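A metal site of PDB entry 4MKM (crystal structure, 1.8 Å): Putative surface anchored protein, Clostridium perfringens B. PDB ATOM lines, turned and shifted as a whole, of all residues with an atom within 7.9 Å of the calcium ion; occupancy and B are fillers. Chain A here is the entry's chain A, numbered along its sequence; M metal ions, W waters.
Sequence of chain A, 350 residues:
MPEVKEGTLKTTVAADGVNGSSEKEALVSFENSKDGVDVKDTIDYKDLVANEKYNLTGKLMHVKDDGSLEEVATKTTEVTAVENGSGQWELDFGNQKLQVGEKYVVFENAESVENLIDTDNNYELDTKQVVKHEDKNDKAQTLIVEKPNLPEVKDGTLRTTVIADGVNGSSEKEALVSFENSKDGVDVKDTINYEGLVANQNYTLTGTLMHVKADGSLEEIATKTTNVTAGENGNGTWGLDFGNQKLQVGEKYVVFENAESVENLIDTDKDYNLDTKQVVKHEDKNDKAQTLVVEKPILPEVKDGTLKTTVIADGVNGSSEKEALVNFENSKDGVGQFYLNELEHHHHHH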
ATOM      1  N   ALA A 164      -7.763  -7.989   6.863  1.00  0.00           N
ATOM      2  CA  ALA A 164      -6.424  -8.325   6.372  1.00  0.00           C
ATOM      3  C   ALA A 164      -5.354  -7.667   7.308  1.00  0.00           C
ATOM      4  O   ALA A 164      -5.312  -6.442   7.415  1.00  0.00           O
ATOM      5  CB  ALA A 164      -6.287  -7.834   4.940  1.00  0.00           C
ATOM      6  N   ASP A 165      -4.583  -8.502   8.087  1.00  0.00           N
ATOM      7  CA  ASP A 165      -3.607  -8.043   9.070  1.00  0.00           C
ATOM      8  C   ASP A 165      -4.265  -7.018  10.026  1.00  0.00           C
ATOM      9  O   ASP A 165      -3.733  -5.941  10.244  1.00  0.00           O
ATOM     10  CB  ASP A 165      -2.322  -7.538   8.392  1.00  0.00           C
ATOM     11  CG  ASP A 165      -1.256  -8.606   8.154  1.00  0.00           C
ATOM     12  OD1 ASP A 165      -1.363  -9.693   8.762  1.00  0.00           O
ATOM     13  OD2 ASP A 165      -0.268  -8.308   7.450  1.00  0.00           O
ATOM     14  N   GLY A 166      -5.472  -7.382  10.510  1.00  0.00           N
ATOM     15  CA  GLY A 166      -6.283  -6.586  11.439  1.00  0.00           C
ATOM     16  C   GLY A 166      -6.989  -5.372  10.846  1.00  0.00           C
ATOM     17  O   GLY A 166      -7.565  -4.586  11.600  1.00  0.00           O
ATOM     18  N   VAL A 177      -3.040  -3.211   3.365  1.00  0.00           N
ATOM     19  CA  VAL A 177      -2.025  -3.904   4.157  1.00  0.00           C
ATOM     20  C   VAL A 177      -0.679  -3.223   3.853  1.00  0.00           C
ATOM     21  O   VAL A 177      -0.169  -3.321   2.732  1.00  0.00           O
ATOM     22  CB  VAL A 177      -1.990  -5.410   3.815  1.00  0.00           C
ATOM     23  CG1 VAL A 177      -0.937  -6.146   4.656  1.00  0.00           C
ATOM     24  CG2 VAL A 177      -3.351  -6.041   4.004  1.00  0.00           C
ATOM     25  N   SER A 178      -0.100  -2.540   4.849  1.00  0.00           N
ATOM     26  CA  SER A 178       1.223  -1.893   4.683  1.00  0.00           C
ATOM     27  C   SER A 178       2.284  -2.919   4.303  1.00  0.00           C
ATOM     28  O   SER A 178       2.130  -4.097   4.623  1.00  0.00           O
ATOM     29  CB  SER A 178       1.631  -1.196   5.981  1.00  0.00           C
ATOM     30  OG  SER A 178       1.923  -2.117   7.014  1.00  0.00           O
ATOM     31  N   PHE A 179       3.408  -2.443   3.682  1.00  0.00           N
ATOM     32  CA  PHE A 179       4.530  -3.318   3.317  1.00  0.00           C
ATOM     33  C   PHE A 179       5.102  -3.999   4.579  1.00  0.00           C
ATOM     34  O   PHE A 179       5.317  -5.208   4.547  1.00  0.00           O
ATOM     35  CB  PHE A 179       5.616  -2.542   2.552  1.00  0.00           C
ATOM     36  CG  PHE A 179       6.849  -3.370   2.253  1.00  0.00           C
ATOM     37  CD1 PHE A 179       6.795  -4.415   1.350  1.00  0.00           C
ATOM     38  CD2 PHE A 179       8.023  -3.152   2.935  1.00  0.00           C
ATOM     39  CE1 PHE A 179       7.909  -5.202   1.108  1.00  0.00           C
ATOM     40  CE2 PHE A 179       9.141  -3.947   2.694  1.00  0.00           C
ATOM     41  CZ  PHE A 179       9.077  -4.966   1.769  1.00  0.00           C
ATOM     42  N   GLU A 180       5.263  -3.231   5.682  1.00  0.00           N
ATOM     43  CA  GLU A 180       5.735  -3.758   6.977  1.00  0.00           C
ATOM     44  C   GLU A 180       4.846  -4.952   7.397  1.00  0.00           C
ATOM     45  O   GLU A 180       5.348  -6.034   7.705  1.00  0.00           O
ATOM     46  CB  GLU A 180       5.659  -2.642   8.059  1.00  0.00           C
ATOM     47  CG  GLU A 180       6.216  -2.984   9.437  1.00  0.00           C
ATOM     48  CD  GLU A 180       7.723  -3.098   9.518  1.00  0.00           C
ATOM     49  OE1 GLU A 180       8.392  -2.076   9.794  1.00  0.00           O
ATOM     50  OE2 GLU A 180       8.242  -4.229   9.348  1.00  0.00           O
ATOM     51  N   ASN A 181       3.540  -4.754   7.361  1.00  0.00           N
ATOM     52  CA  ASN A 181       2.590  -5.831   7.688  1.00  0.00           C
ATOM     53  C   ASN A 181       2.749  -7.054   6.786  1.00  0.00           C
ATOM     54  O   ASN A 181       2.747  -8.161   7.293  1.00  0.00           O
ATOM     55  CB  ASN A 181       1.162  -5.291   7.715  1.00  0.00           C
ATOM     56  CG  ASN A 181       0.669  -4.881   9.092  1.00  0.00           C
ATOM     57  OD1 ASN A 181       1.052  -5.452  10.111  1.00  0.00           O
ATOM     58  ND2 ASN A 181      -0.320  -4.009   9.137  1.00  0.00           N
ATOM     59  N   SER A 182       2.989  -6.863   5.471  1.00  0.00           N
ATOM     60  CA  SER A 182       3.136  -8.002   4.557  1.00  0.00           C
ATOM     61  C   SER A 182       4.348  -8.920   4.753  1.00  0.00           C
ATOM     62  O   SER A 182       4.245 -10.089   4.399  1.00  0.00           O
ATOM     63  CB  SER A 182       3.086  -7.528   3.105  1.00  0.00           C
ATOM     64  OG  SER A 182       4.330  -7.036   2.643  1.00  0.00           O
ATOM     65  N   LYS A 183       5.470  -8.400   5.287  1.00  0.00           N
ATOM     66  CA  LYS A 183       6.755  -9.107   5.442  1.00  0.00           C
ATOM     67  C   LYS A 183       6.650 -10.526   6.074  1.00  0.00           C
ATOM     68  O   LYS A 183       7.385 -11.430   5.668  1.00  0.00           O
ATOM     69  CB  LYS A 183       7.703  -8.259   6.315  1.00  0.00           C
ATOM     70  CG  LYS A 183       8.160  -6.952   5.673  1.00  0.00           C
ATOM     71  CD  LYS A 183       9.321  -6.336   6.473  1.00  0.00           C
ATOM     72  CE  LYS A 183       9.696  -4.942   6.021  1.00  0.00           C
ATOM     73  NZ  LYS A 183      10.381  -4.189   7.102  1.00  0.00           N
ATOM     74  N   ASP A 184       5.781 -10.679   7.083  1.00  0.00           N
ATOM     75  CA  ASP A 184       5.544 -11.973   7.761  1.00  0.00           C
ATOM     76  C   ASP A 184       4.219 -12.660   7.303  1.00  0.00           C
ATOM     77  O   ASP A 184       3.608 -13.405   8.088  1.00  0.00           O
ATOM     78  CB  ASP A 184       5.538 -11.766   9.298  1.00  0.00           C
ATOM     79  CG  ASP A 184       4.414 -10.920   9.855  1.00  0.00           C
ATOM     80  OD1 ASP A 184       3.777 -10.170   9.073  1.00  0.00           O
ATOM     81  OD2 ASP A 184       4.159 -11.013  11.078  1.00  0.00           O
ATOM     82  N   GLY A 185       3.780 -12.374   6.071  1.00  0.00           N
ATOM     83  CA  GLY A 185       2.534 -12.929   5.550  1.00  0.00           C
ATOM     84  C   GLY A 185       1.348 -12.073   5.982  1.00  0.00           C
ATOM     85  O   GLY A 185       1.522 -11.122   6.755  1.00  0.00           O
ATOM     86  N   VAL A 186       0.152 -12.370   5.447  1.00  0.00           N
ATOM     87  CA  VAL A 186      -1.045 -11.593   5.722  1.00  0.00           C
ATOM     88  C   VAL A 186      -2.089 -12.499   6.330  1.00  0.00           C
ATOM     89  O   VAL A 186      -2.473 -13.496   5.716  1.00  0.00           O
ATOM     90  CB  VAL A 186      -1.588 -10.883   4.467  1.00  0.00           C
ATOM     91  CG1 VAL A 186      -2.746  -9.961   4.814  1.00  0.00           C
ATOM     92  CG2 VAL A 186      -0.476 -10.111   3.748  1.00  0.00           C
ATOM     93  N   ASP A 187      -2.520 -12.196   7.554  1.00  0.00           N
ATOM     94  CA  ASP A 187      -3.559 -12.967   8.207  1.00  0.00           C
ATOM     95  C   ASP A 187      -4.859 -12.513   7.574  1.00  0.00           C
ATOM     96  O   ASP A 187      -5.156 -11.327   7.608  1.00  0.00           O
ATOM     97  CB  ASP A 187      -3.521 -12.749   9.733  1.00  0.00           C
ATOM     98  CG  ASP A 187      -2.177 -13.186  10.283  1.00  0.00           C
ATOM     99  OD1 ASP A 187      -1.713 -14.278   9.888  1.00  0.00           O
ATOM    100  OD2 ASP A 187      -1.541 -12.380  11.018  1.00  0.00           O
ATOM    101  N   ASN A 244      -2.604 -17.460   7.760  1.00  0.00           N
ATOM    102  CA  ASN A 244      -1.512 -16.633   7.252  1.00  0.00           C
ATOM    103  C   ASN A 244      -1.290 -16.929   5.779  1.00  0.00           C
ATOM    104  O   ASN A 244      -1.060 -18.081   5.425  1.00  0.00           O
ATOM    105  CB  ASN A 244      -0.218 -16.865   8.062  1.00  0.00           C
ATOM    106  CG  ASN A 244       0.845 -15.888   7.705  1.00  0.00           C
ATOM    107  OD1 ASN A 244       1.636 -16.130   6.773  1.00  0.00           O
ATOM    108  ND2 ASN A 244       0.823 -14.729   8.329  1.00  0.00           N
ATOM    109  N   GLN A 245      -1.379 -15.897   4.924  1.00  0.00           N
ATOM    110  CA  GLN A 245      -1.242 -16.056   3.467  1.00  0.00           C
ATOM    111  C   GLN A 245      -0.023 -15.351   2.974  1.00  0.00           C
ATOM    112  O   GLN A 245       0.221 -14.222   3.387  1.00  0.00           O
ATOM    113  CB  GLN A 245      -2.486 -15.472   2.767  1.00  0.00           C
ATOM    114  CG  GLN A 245      -3.826 -16.184   3.072  1.00  0.00           C
ATOM    115  CD  GLN A 245      -3.839 -17.615   2.588  1.00  0.00           C
ATOM    116  OE1 GLN A 245      -3.321 -17.923   1.515  1.00  0.00           O
ATOM    117  NE2 GLN A 245      -4.363 -18.542   3.367  1.00  0.00           N
ATOM    118  N   LYS A 246       0.747 -15.984   2.060  1.00  0.00           N
ATOM    119  CA  LYS A 246       1.976 -15.394   1.514  1.00  0.00           C
ATOM    120  C   LYS A 246       1.631 -14.595   0.252  1.00  0.00           C
ATOM    121  O   LYS A 246       1.908 -14.976  -0.873  1.00  0.00           O
ATOM    122  CB  LYS A 246       3.015 -16.490   1.261  1.00  0.00           C
ATOM    123  CG  LYS A 246       3.326 -17.331   2.525  1.00  0.00           C
ATOM    124  CD  LYS A 246       3.709 -16.492   3.769  1.00  0.00           C
ATOM    125  CE  LYS A 246       4.049 -17.322   4.978  1.00  0.00           C
ATOM    126  NZ  LYS A 246       4.460 -16.476   6.136  1.00  0.00           N
HETATM  127 CA    CA M   1       1.312  -9.652   8.450  1.00  0.00          CA
HETATM  128  O   HOH W   1       1.147  -8.279  10.305  1.00  0.00           O
HETATM  129  O   HOH W   2       1.228 -11.247   9.400  1.00  0.00           O
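Of the 17 residues printed, 4 come within 4 Å of the calcium ion.
The calcium ion is bound by water W2 (1.9 Å), the backbone carbonyl oxygen (O) of Gly 185 (2.3 Å), the side-chain carboxylate (OD2) of Asp 165 (2.3 Å), water W1 (2.3 Å), the backbone carbonyl oxygen (O) of Asn 181 (2.4 Å), the side-chain carboxylate (OD1) of Asp 184 (2.6 Å) and the side-chain carboxylate (OD1) of Asp 165 (2.7 Å). The calcium ion has seven donor atoms within binding distance.
Water W2 lies within hydrogen-bond range of the side-chain carboxylate of Asp 184 and the side-chain carboxylate of Asp 187.
The backbone NH (N) of Asp 165 sits at hydrogen-bond distance from the backbone carbonyl oxygen (O) of Asp 187. N of Asn 181 sits at hydrogen-bond distance from OG of Ser 178 (3.1 Å). The backbone carbonyl oxygen of Asp 184 lies within hydrogen-bond range of the side-chain amide nitrogen of Asn 244 (3.1 Å).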
